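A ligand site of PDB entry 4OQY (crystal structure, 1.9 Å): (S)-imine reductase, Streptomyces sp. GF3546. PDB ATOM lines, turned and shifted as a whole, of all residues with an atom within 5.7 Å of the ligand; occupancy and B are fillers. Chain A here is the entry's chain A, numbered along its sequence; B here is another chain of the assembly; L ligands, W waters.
The backbone NH (N) of Thr 68 lies within hydrogen-bond range of an oxygen (O4) of the ligand (3.1 Å).
O12 of the ligand is in hydrogen-bond range of O of Thr 68 (2.9 Å).
An oxygen (O3) of the ligand sits at hydrogen-bond distance from the side-chain hydroxyl (OG1) of Thr 68, at 2.6 Å.
N of Thr 35 lies within hydrogen-bond range of O15 of the ligand (3.1 Å).
OG1 of Thr 35 sits at hydrogen-bond distance from O15 of the ligand.
An oxygen (O5) of the ligand sits at hydrogen-bond distance from the side-chain amide oxygen (OD1) of Asn 33 (2.7 Å).
NZ of Lys 38 is in salt-bridge range of O16 of the ligand (2.7 Å).
O17 of the ligand lies within salt-bridge range of NH2 of Arg 34 (2.8 Å).
An oxygen (O12) of the ligand lies within hydrogen-bond range of the backbone NH (N) of Ser 94 (2.9 Å).
An oxygen (O13) of the ligand lies within hydrogen-bond range of the side-chain hydroxyl (OG) of Ser 94 (2.9 Å).
O12 of the ligand is in hydrogen-bond range of O of Leu 67.
O9 of the ligand is in hydrogen-bond range of N of Met 14.
An oxygen (O5) of the ligand lies within hydrogen-bond range of the backbone NH (N) of Leu 11 (3.3 Å).
N of Pro 13 lies close to O9 of the ligand (3.3 Å).
CA of Gly 10 touches O5 of the ligand (3.4 Å).
Gly 12 touches the ligand (C to O9, 3.5 Å).
OG of Ser 66 touches C11 of the ligand, at 3.8 Å.
Ala 72 touches the ligand.
Ile 76 touches the ligand.
CA of Ser 93 touches O12 of the ligand, at 3.7 Å.
Val 119 touches the ligand.
O of Val 121 touches C19 of the ligand (3.1 Å).
Pro 122 touches the ligand (CA to O14, 3.4 Å).
CD of Pro 123 touches O14 of the ligand, at 3.5 Å.
OH of Tyr 169 touches C21 of the ligand, at 3.9 Å.
The nearest printed residue that does not touch the ligand is Ala 75 (4.1 Å).
O of Thr 35 lies within hydrogen-bond range of ND2 of Asn 33.
N of Leu 11 sits at hydrogen-bond distance from OD1 of Asn 33 (2.9 Å).
OG of Ser 93 is in hydrogen-bond range of N of Leu 67, 3.1 Å away.
The backbone NH (N) of Ala 72 is in hydrogen-bond range of the side-chain carboxylate (OD1) of Asp 69 (3.1 Å).
The side-chain hydroxyl (OG) of Ser 66 lies within hydrogen-bond range of the backbone NH (N) of Gly 15, at 3.5 Å.
Water W1 lies within hydrogen-bond range of O9 of the ligand (2.6 Å), N of Gly 15 (2.9 Å), O of Ser 66 (3.0 Å) and N of Gly 12 (3.1 Å).
Water W3 lies within hydrogen-bond range of O of Leu 92 (2.7 Å), O11 of the ligand (2.9 Å) and OG of Ser 66 (3.1 Å).
Water W2 lies within hydrogen-bond range of OD1 of Asn 33 (2.8 Å), N of Arg 34 (2.9 Å) and N5 of the ligand (3.3 Å).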
ATOM      1  N   GLY A  10      -3.978  -1.433  -3.015  1.00  0.00           N
ATOM      2  CA  GLY A  10      -3.850  -1.747  -4.439  1.00  0.00           C
ATOM      3  C   GLY A  10      -4.879  -2.754  -4.882  1.00  0.00           C
ATOM      4  O   GLY A  10      -4.821  -3.929  -4.490  1.00  0.00           O
ATOM      5  N   LEU A  11      -5.861  -2.279  -5.614  1.00  0.00           N
ATOM      6  CA  LEU A  11      -7.012  -3.039  -6.036  1.00  0.00           C
ATOM      7  C   LEU A  11      -7.140  -3.123  -7.552  1.00  0.00           C
ATOM      8  O   LEU A  11      -8.234  -3.069  -8.094  1.00  0.00           O
ATOM      9  CB  LEU A  11      -8.276  -2.408  -5.457  1.00  0.00           C
ATOM     10  CG  LEU A  11      -8.281  -2.260  -3.935  1.00  0.00           C
ATOM     11  CD1 LEU A  11      -9.535  -1.538  -3.490  1.00  0.00           C
ATOM     12  CD2 LEU A  11      -8.122  -3.612  -3.249  1.00  0.00           C
ATOM     13  N   GLY A  12      -6.009  -3.256  -8.243  1.00  0.00           N
ATOM     14  CA  GLY A  12      -6.013  -3.807  -9.581  1.00  0.00           C
ATOM     15  C   GLY A  12      -6.445  -5.292  -9.559  1.00  0.00           C
ATOM     16  O   GLY A  12      -6.854  -5.809  -8.518  1.00  0.00           O
ATOM     17  N   PRO A  13      -6.341  -5.959 -10.711  1.00  0.00           N
ATOM     18  CA  PRO A  13      -6.838  -7.304 -10.805  1.00  0.00           C
ATOM     19  C   PRO A  13      -6.218  -8.257  -9.754  1.00  0.00           C
ATOM     20  O   PRO A  13      -6.934  -9.057  -9.187  1.00  0.00           O
ATOM     21  CB  PRO A  13      -6.504  -7.703 -12.239  1.00  0.00           C
ATOM     22  CG  PRO A  13      -6.556  -6.412 -13.009  1.00  0.00           C
ATOM     23  CD  PRO A  13      -6.132  -5.341 -12.042  1.00  0.00           C
ATOM     24  N   MET A  14      -4.921  -8.127  -9.480  1.00  0.00           N
ATOM     25  CA  MET A  14      -4.267  -8.931  -8.460  1.00  0.00           C
ATOM     26  C   MET A  14      -4.815  -8.665  -7.024  1.00  0.00           C
ATOM     27  O   MET A  14      -5.188  -9.614  -6.282  1.00  0.00           O
ATOM     28  CB  MET A  14      -2.769  -8.691  -8.513  1.00  0.00           C
ATOM     29  CG  MET A  14      -1.984  -9.644  -7.641  1.00  0.00           C
ATOM     30  SD  MET A  14      -2.007 -11.384  -8.154  1.00  0.00           S
ATOM     31  CE  MET A  14      -1.643 -11.342  -9.900  1.00  0.00           C
ATOM     32  N   GLY A  15      -4.844  -7.385  -6.641  1.00  0.00           N
ATOM     33  CA  GLY A  15      -5.416  -6.927  -5.385  1.00  0.00           C
ATOM     34  C   GLY A  15      -6.847  -7.415  -5.147  1.00  0.00           C
ATOM     35  O   GLY A  15      -7.149  -7.947  -4.081  1.00  0.00           O
ATOM     36  N   ASN A  33      -7.317   2.134  -2.120  1.00  0.00           N
ATOM     37  CA  ASN A  33      -6.851   2.264  -3.496  1.00  0.00           C
ATOM     38  C   ASN A  33      -6.874   3.742  -3.948  1.00  0.00           C
ATOM     39  O   ASN A  33      -7.692   4.546  -3.515  1.00  0.00           O
ATOM     40  CB  ASN A  33      -7.702   1.406  -4.415  1.00  0.00           C
ATOM     41  CG  ASN A  33      -7.030   1.148  -5.774  1.00  0.00           C
ATOM     42  OD1 ASN A  33      -5.906   0.631  -5.846  1.00  0.00           O
ATOM     43  ND2 ASN A  33      -7.706   1.523  -6.850  1.00  0.00           N
ATOM     44  N   ARG A  34      -5.937   4.091  -4.821  1.00  0.00           N
ATOM     45  CA  ARG A  34      -5.891   5.456  -5.360  1.00  0.00           C
ATOM     46  C   ARG A  34      -7.232   5.813  -6.016  1.00  0.00           C
ATOM     47  O   ARG A  34      -7.774   6.895  -5.809  1.00  0.00           O
ATOM     48  CB  ARG A  34      -4.762   5.601  -6.399  1.00  0.00           C
ATOM     49  CG  ARG A  34      -4.947   6.718  -7.427  1.00  0.00           C
ATOM     50  CD  ARG A  34      -3.750   6.846  -8.366  1.00  0.00           C
ATOM     51  NE  ARG A  34      -3.656   5.721  -9.298  1.00  0.00           N
ATOM     52  CZ  ARG A  34      -2.763   5.629 -10.289  1.00  0.00           C
ATOM     53  NH1 ARG A  34      -1.867   6.591 -10.521  1.00  0.00           N
ATOM     54  NH2 ARG A  34      -2.769   4.558 -11.075  1.00  0.00           N
ATOM     55  N   THR A  35      -7.765   4.869  -6.782  1.00  0.00           N
ATOM     56  CA  THR A  35      -9.075   5.022  -7.369  1.00  0.00           C
ATOM     57  C   THR A  35     -10.080   4.287  -6.492  1.00  0.00           C
ATOM     58  O   THR A  35     -10.228   3.061  -6.582  1.00  0.00           O
ATOM     59  CB  THR A  35      -9.138   4.487  -8.804  1.00  0.00           C
ATOM     60  OG1 THR A  35      -8.068   5.048  -9.576  1.00  0.00           O
ATOM     61  CG2 THR A  35     -10.449   4.875  -9.439  1.00  0.00           C
ATOM     62  N   LYS A  38     -12.937   1.490  -7.394  1.00  0.00           N
ATOM     63  CA  LYS A  38     -12.582   0.108  -7.621  1.00  0.00           C
ATOM     64  C   LYS A  38     -12.820  -0.782  -6.408  1.00  0.00           C
ATOM     65  O   LYS A  38     -12.696  -1.985  -6.522  1.00  0.00           O
ATOM     66  CB  LYS A  38     -11.142  -0.006  -8.065  1.00  0.00           C
ATOM     67  CG  LYS A  38     -10.930   0.650  -9.416  1.00  0.00           C
ATOM     68  CD  LYS A  38      -9.737   0.052 -10.111  1.00  0.00           C
ATOM     69  CE  LYS A  38      -9.423   0.831 -11.370  1.00  0.00           C
ATOM     70  NZ  LYS A  38      -7.968   0.720 -11.649  1.00  0.00           N
ATOM     71  N   SER A  66      -0.233  -4.674  -3.395  1.00  0.00           N
ATOM     72  CA  SER A  66      -0.328  -5.207  -4.743  1.00  0.00           C
ATOM     73  C   SER A  66      -0.409  -4.014  -5.703  1.00  0.00           C
ATOM     74  O   SER A  66      -1.483  -3.624  -6.134  1.00  0.00           O
ATOM     75  CB  SER A  66      -1.547  -6.062  -4.931  1.00  0.00           C
ATOM     76  OG  SER A  66      -1.449  -6.726  -6.183  1.00  0.00           O
ATOM     77  N   LEU A  67       0.739  -3.434  -5.982  1.00  0.00           N
ATOM     78  CA  LEU A  67       0.803  -2.201  -6.795  1.00  0.00           C
ATOM     79  C   LEU A  67       1.648  -2.420  -8.025  1.00  0.00           C
ATOM     80  O   LEU A  67       2.361  -3.424  -8.138  1.00  0.00           O
ATOM     81  CB  LEU A  67       1.336  -1.058  -5.949  1.00  0.00           C
ATOM     82  CG  LEU A  67       0.429  -0.682  -4.779  1.00  0.00           C
ATOM     83  CD1 LEU A  67       1.162   0.092  -3.690  1.00  0.00           C
ATOM     84  CD2 LEU A  67      -0.779   0.105  -5.245  1.00  0.00           C
ATOM     85  N   THR A  68       1.592  -1.474  -8.975  1.00  0.00           N
ATOM     86  CA  THR A  68       2.177  -1.753 -10.254  1.00  0.00           C
ATOM     87  C   THR A  68       3.678  -1.910 -10.124  1.00  0.00           C
ATOM     88  O   THR A  68       4.246  -2.765 -10.777  1.00  0.00           O
ATOM     89  CB  THR A  68       1.811  -0.705 -11.317  1.00  0.00           C
ATOM     90  OG1 THR A  68       0.395  -0.509 -11.283  1.00  0.00           O
ATOM     91  CG2 THR A  68       2.155  -1.204 -12.700  1.00  0.00           C
ATOM     92  N   ASP A  69       4.328  -1.100  -9.292  1.00  0.00           N
ATOM     93  CA  ASP A  69       5.796  -1.148  -9.145  1.00  0.00           C
ATOM     94  C   ASP A  69       6.224  -0.377  -7.906  1.00  0.00           C
ATOM     95  O   ASP A  69       5.383   0.183  -7.216  1.00  0.00           O
ATOM     96  CB  ASP A  69       6.489  -0.603 -10.418  1.00  0.00           C
ATOM     97  CG  ASP A  69       6.109   0.832 -10.766  1.00  0.00           C
ATOM     98  OD1 ASP A  69       5.681   1.620  -9.882  1.00  0.00           O
ATOM     99  OD2 ASP A  69       6.289   1.189 -11.949  1.00  0.00           O
ATOM    100  N   ASP A  71       7.703   2.588  -7.578  1.00  0.00           N
ATOM    101  CA  ASP A  71       7.337   3.990  -7.688  1.00  0.00           C
ATOM    102  C   ASP A  71       5.947   4.197  -7.083  1.00  0.00           C
ATOM    103  O   ASP A  71       5.725   5.147  -6.339  1.00  0.00           O
ATOM    104  CB  ASP A  71       7.304   4.463  -9.150  1.00  0.00           C
ATOM    105  CG  ASP A  71       8.696   4.720  -9.750  1.00  0.00           C
ATOM    106  OD1 ASP A  71       9.700   4.924  -9.038  1.00  0.00           O
ATOM    107  OD2 ASP A  71       8.770   4.699 -10.973  1.00  0.00           O
ATOM    108  N   ALA A  72       5.014   3.294  -7.393  1.00  0.00           N
ATOM    109  CA  ALA A  72       3.645   3.324  -6.828  1.00  0.00           C
ATOM    110  C   ALA A  72       3.621   3.109  -5.312  1.00  0.00           C
ATOM    111  O   ALA A  72       2.877   3.762  -4.587  1.00  0.00           O
ATOM    112  CB  ALA A  72       2.775   2.287  -7.508  1.00  0.00           C
ATOM    113  N   ALA A  75       4.895   6.280  -3.686  1.00  0.00           N
ATOM    114  CA  ALA A  75       3.911   7.346  -3.831  1.00  0.00           C
ATOM    115  C   ALA A  75       2.855   7.253  -2.738  1.00  0.00           C
ATOM    116  O   ALA A  75       2.430   8.251  -2.182  1.00  0.00           O
ATOM    117  CB  ALA A  75       3.266   7.297  -5.186  1.00  0.00           C
ATOM    118  N   ILE A  76       2.431   6.038  -2.425  1.00  0.00           N
ATOM    119  CA  ILE A  76       1.469   5.828  -1.341  1.00  0.00           C
ATOM    120  C   ILE A  76       2.071   5.920   0.060  1.00  0.00           C
ATOM    121  O   ILE A  76       1.455   6.491   0.958  1.00  0.00           O
ATOM    122  CB  ILE A  76       0.732   4.492  -1.541  1.00  0.00           C
ATOM    123  CG1 ILE A  76      -0.117   4.605  -2.804  1.00  0.00           C
ATOM    124  CG2 ILE A  76      -0.128   4.142  -0.321  1.00  0.00           C
ATOM    125  CD1 ILE A  76      -0.689   3.321  -3.340  1.00  0.00           C
ATOM    126  N   LEU A  92       4.004  -7.358  -2.532  1.00  0.00           N
ATOM    127  CA  LEU A  92       3.880  -8.274  -3.663  1.00  0.00           C
ATOM    128  C   LEU A  92       3.902  -7.549  -4.999  1.00  0.00           C
ATOM    129  O   LEU A  92       3.502  -8.118  -6.003  1.00  0.00           O
ATOM    130  CB  LEU A  92       2.607  -9.128  -3.592  1.00  0.00           C
ATOM    131  CG  LEU A  92       2.632 -10.336  -2.630  1.00  0.00           C
ATOM    132  CD1 LEU A  92       3.488 -10.155  -1.385  1.00  0.00           C
ATOM    133  CD2 LEU A  92       1.232 -10.763  -2.249  1.00  0.00           C
ATOM    134  N   SER A  93       4.386  -6.315  -5.000  1.00  0.00           N
ATOM    135  CA  SER A  93       4.530  -5.520  -6.232  1.00  0.00           C
ATOM    136  C   SER A  93       5.826  -5.950  -6.931  1.00  0.00           C
ATOM    137  O   SER A  93       6.869  -6.043  -6.297  1.00  0.00           O
ATOM    138  CB  SER A  93       4.644  -4.037  -5.889  1.00  0.00           C
ATOM    139  OG  SER A  93       3.666  -3.547  -5.005  1.00  0.00           O
ATOM    140  N   SER A  94       5.785  -6.208  -8.227  1.00  0.00           N
ATOM    141  CA  SER A  94       6.980  -6.716  -8.893  1.00  0.00           C
ATOM    142  C   SER A  94       7.889  -5.535  -9.334  1.00  0.00           C
ATOM    143  O   SER A  94       7.414  -4.525  -9.827  1.00  0.00           O
ATOM    144  CB  SER A  94       6.591  -7.651 -10.043  1.00  0.00           C
ATOM    145  OG  SER A  94       6.267  -6.948 -11.209  1.00  0.00           O
ATOM    146  N   VAL A 119       4.848 -13.014  -6.991  1.00  0.00           N
ATOM    147  CA  VAL A 119       3.675 -13.851  -7.267  1.00  0.00           C
ATOM    148  C   VAL A 119       3.888 -14.496  -8.618  1.00  0.00           C
ATOM    149  O   VAL A 119       4.225 -13.829  -9.579  1.00  0.00           O
ATOM    150  CB  VAL A 119       2.341 -13.082  -7.199  1.00  0.00           C
ATOM    151  CG1 VAL A 119       1.142 -13.983  -7.518  1.00  0.00           C
ATOM    152  CG2 VAL A 119       2.184 -12.445  -5.827  1.00  0.00           C
ATOM    153  N   GLN A 120       3.729 -15.823  -8.688  1.00  0.00           N
ATOM    154  CA  GLN A 120       4.113 -16.552  -9.896  1.00  0.00           C
ATOM    155  C   GLN A 120       2.977 -16.765 -10.863  1.00  0.00           C
ATOM    156  O   GLN A 120       3.200 -17.303 -11.939  1.00  0.00           O
ATOM    157  CB  GLN A 120       4.695 -17.903  -9.534  1.00  0.00           C
ATOM    158  CG  GLN A 120       5.968 -17.845  -8.736  1.00  0.00           C
ATOM    159  CD  GLN A 120       6.243 -19.162  -8.027  1.00  0.00           C
ATOM    160  OE1 GLN A 120       5.850 -20.220  -8.519  1.00  0.00           O
ATOM    161  NE2 GLN A 120       6.829 -19.095  -6.853  1.00  0.00           N
ATOM    162  N   VAL A 121       1.779 -16.335 -10.483  1.00  0.00           N
ATOM    163  CA  VAL A 121       0.553 -16.678 -11.204  1.00  0.00           C
ATOM    164  C   VAL A 121      -0.320 -15.474 -11.420  1.00  0.00           C
ATOM    165  O   VAL A 121      -0.233 -14.516 -10.664  1.00  0.00           O
ATOM    166  CB  VAL A 121      -0.324 -17.678 -10.400  1.00  0.00           C
ATOM    167  CG1 VAL A 121       0.388 -19.014 -10.268  1.00  0.00           C
ATOM    168  CG2 VAL A 121      -0.703 -17.115  -9.041  1.00  0.00           C
ATOM    169  N   PRO A 122      -1.214 -15.554 -12.409  1.00  0.00           N
ATOM    170  CA  PRO A 122      -2.169 -14.474 -12.655  1.00  0.00           C
ATOM    171  C   PRO A 122      -3.318 -14.511 -11.663  1.00  0.00           C
ATOM    172  O   PRO A 122      -3.531 -15.527 -11.001  1.00  0.00           O
ATOM    173  CB  PRO A 122      -2.658 -14.747 -14.085  1.00  0.00           C
ATOM    174  CG  PRO A 122      -2.580 -16.233 -14.188  1.00  0.00           C
ATOM    175  CD  PRO A 122      -1.312 -16.589 -13.454  1.00  0.00           C
ATOM    176  N   PRO A 123      -4.088 -13.425 -11.596  1.00  0.00           N
ATOM    177  CA  PRO A 123      -5.110 -13.316 -10.569  1.00  0.00           C
ATOM    178  C   PRO A 123      -6.069 -14.486 -10.397  1.00  0.00           C
ATOM    179  O   PRO A 123      -6.393 -14.779  -9.264  1.00  0.00           O
ATOM    180  CB  PRO A 123      -5.855 -12.050 -10.960  1.00  0.00           C
ATOM    181  CG  PRO A 123      -4.795 -11.216 -11.599  1.00  0.00           C
ATOM    182  CD  PRO A 123      -3.998 -12.190 -12.391  1.00  0.00           C
ATOM    183  N   TYR A 169      11.539 -13.921  -9.356  1.00  0.00           N
ATOM    184  CA  TYR A 169      10.455 -13.456 -10.226  1.00  0.00           C
ATOM    185  C   TYR A 169      11.022 -12.970 -11.558  1.00  0.00           C
ATOM    186  O   TYR A 169      10.506 -13.306 -12.622  1.00  0.00           O
ATOM    187  CB  TYR A 169       9.587 -12.364  -9.545  1.00  0.00           C
ATOM    188  CG  TYR A 169       8.485 -11.843 -10.456  1.00  0.00           C
ATOM    189  CD1 TYR A 169       7.258 -12.493 -10.544  1.00  0.00           C
ATOM    190  CD2 TYR A 169       8.689 -10.713 -11.252  1.00  0.00           C
ATOM    191  CE1 TYR A 169       6.268 -12.019 -11.401  1.00  0.00           C
ATOM    192  CE2 TYR A 169       7.719 -10.248 -12.109  1.00  0.00           C
ATOM    193  CZ  TYR A 169       6.519 -10.916 -12.188  1.00  0.00           C
ATOM    194  OH  TYR A 169       5.585 -10.427 -13.044  1.00  0.00           O
ATOM    195  N   MET B 236       2.266  -3.287 -21.100  1.00  0.00           N
ATOM    196  CA  MET B 236       2.522  -4.004 -19.870  1.00  0.00           C
ATOM    197  C   MET B 236       3.733  -4.916 -20.016  1.00  0.00           C
ATOM    198  O   MET B 236       4.565  -5.021 -19.107  1.00  0.00           O
ATOM    199  CB  MET B 236       1.268  -4.788 -19.446  1.00  0.00           C
ATOM    200  CG  MET B 236       0.042  -3.887 -19.238  1.00  0.00           C
ATOM    201  SD  MET B 236      -0.011  -2.847 -17.727  1.00  0.00           S
ATOM    202  CE  MET B 236       0.958  -1.379 -18.098  1.00  0.00           C
HETATM  203  P1  LIG L   1      -1.085  -3.343 -12.194  1.00  0.00           P
HETATM  204  O1  LIG L   1      -1.554  -2.371 -13.240  1.00  0.00           O
HETATM  205  O2  LIG L   1       0.296  -3.954 -12.327  1.00  0.00           O
HETATM  206  O3  LIG L   1      -1.198  -2.559 -10.767  1.00  0.00           O
HETATM  207  C1  LIG L   1      -2.340  -1.745 -10.502  1.00  0.00           C
HETATM  208  C2  LIG L   1      -2.335  -1.121  -9.107  1.00  0.00           C
HETATM  209  O4  LIG L   1      -1.240  -0.194  -8.932  1.00  0.00           O
HETATM  210  C3  LIG L   1      -3.636  -0.339  -8.919  1.00  0.00           C
HETATM  211  O5  LIG L   1      -4.090  -0.369  -7.563  1.00  0.00           O
HETATM  212  C4  LIG L   1      -3.208   1.057  -9.341  1.00  0.00           C
HETATM  213  O6  LIG L   1      -4.079   2.133  -8.920  1.00  0.00           O
HETATM  214  C5  LIG L   1      -1.820   1.082  -8.691  1.00  0.00           C
HETATM  215  N1  LIG L   1      -0.938   2.164  -9.185  1.00  0.00           N
HETATM  216  C6  LIG L   1      -0.271   2.273 -10.357  1.00  0.00           C
HETATM  217  N2  LIG L   1       0.468   3.431 -10.379  1.00  0.00           N
HETATM  218  C7  LIG L   1       0.259   4.049  -9.195  1.00  0.00           C
HETATM  219  C8  LIG L   1       0.698   5.285  -8.523  1.00  0.00           C
HETATM  220  N3  LIG L   1       1.538   6.141  -9.139  1.00  0.00           N
HETATM  221  N4  LIG L   1       0.226   5.532  -7.272  1.00  0.00           N
HETATM  222  C9  LIG L   1      -0.614   4.694  -6.618  1.00  0.00           C
HETATM  223  N5  LIG L   1      -1.069   3.547  -7.154  1.00  0.00           N
HETATM  224  C10 LIG L   1      -0.666   3.193  -8.408  1.00  0.00           C
HETATM  225  O7  LIG L   1      -2.226  -4.502 -12.076  1.00  0.00           O
HETATM  226  P2  LIG L   1      -2.120  -5.960 -11.348  1.00  0.00           P
HETATM  227  O8  LIG L   1      -2.347  -7.062 -12.363  1.00  0.00           O
HETATM  228  O9  LIG L   1      -3.083  -5.985 -10.185  1.00  0.00           O
HETATM  229  O10 LIG L   1      -0.564  -6.075 -10.914  1.00  0.00           O
HETATM  230  C11 LIG L   1      -0.046  -5.733  -9.621  1.00  0.00           C
HETATM  231  C12 LIG L   1       1.340  -6.356  -9.426  1.00  0.00           C
HETATM  232  O11 LIG L   1       1.365  -7.784  -9.539  1.00  0.00           O
HETATM  233  C13 LIG L   1       2.304  -5.831 -10.506  1.00  0.00           C
HETATM  234  O12 LIG L   1       3.496  -5.452  -9.826  1.00  0.00           O
HETATM  235  C14 LIG L   1       2.448  -7.017 -11.453  1.00  0.00           C
HETATM  236  O13 LIG L   1       3.606  -7.120 -12.261  1.00  0.00           O
HETATM  237  C15 LIG L   1       2.399  -8.185 -10.450  1.00  0.00           C
HETATM  238  N6  LIG L   1       1.993  -9.482 -10.976  1.00  0.00           N
HETATM  239  C16 LIG L   1       0.943  -9.504 -11.808  1.00  0.00           C
HETATM  240  C17 LIG L   1       0.432 -10.687 -12.353  1.00  0.00           C
HETATM  241  C18 LIG L   1      -0.752 -10.620 -13.284  1.00  0.00           C
HETATM  242  O14 LIG L   1      -0.976 -11.589 -13.994  1.00  0.00           O
HETATM  243  N7  LIG L   1      -1.567  -9.553 -13.334  1.00  0.00           N
HETATM  244  C19 LIG L   1       1.067 -12.040 -11.963  1.00  0.00           C
HETATM  245  C20 LIG L   1       2.200 -11.886 -11.038  1.00  0.00           C
HETATM  246  C21 LIG L   1       2.612 -10.627 -10.573  1.00  0.00           C
HETATM  247  P3  LIG L   1      -5.431   2.470  -9.725  1.00  0.00           P
HETATM  248  O15 LIG L   1      -5.887   3.672  -8.949  1.00  0.00           O
HETATM  249  O16 LIG L   1      -6.303   1.223  -9.584  1.00  0.00           O
HETATM  250  O17 LIG L   1      -4.881   2.741 -11.098  1.00  0.00           O
HETATM  251  O   HOH W   1      -3.521  -5.059  -7.828  1.00  0.00           O
HETATM  252  O   HOH W   2      -3.714   2.364  -5.578  1.00  0.00           O
HETATM  253  O   HOH W   3       0.950  -8.624  -6.784  1.00  0.00           O
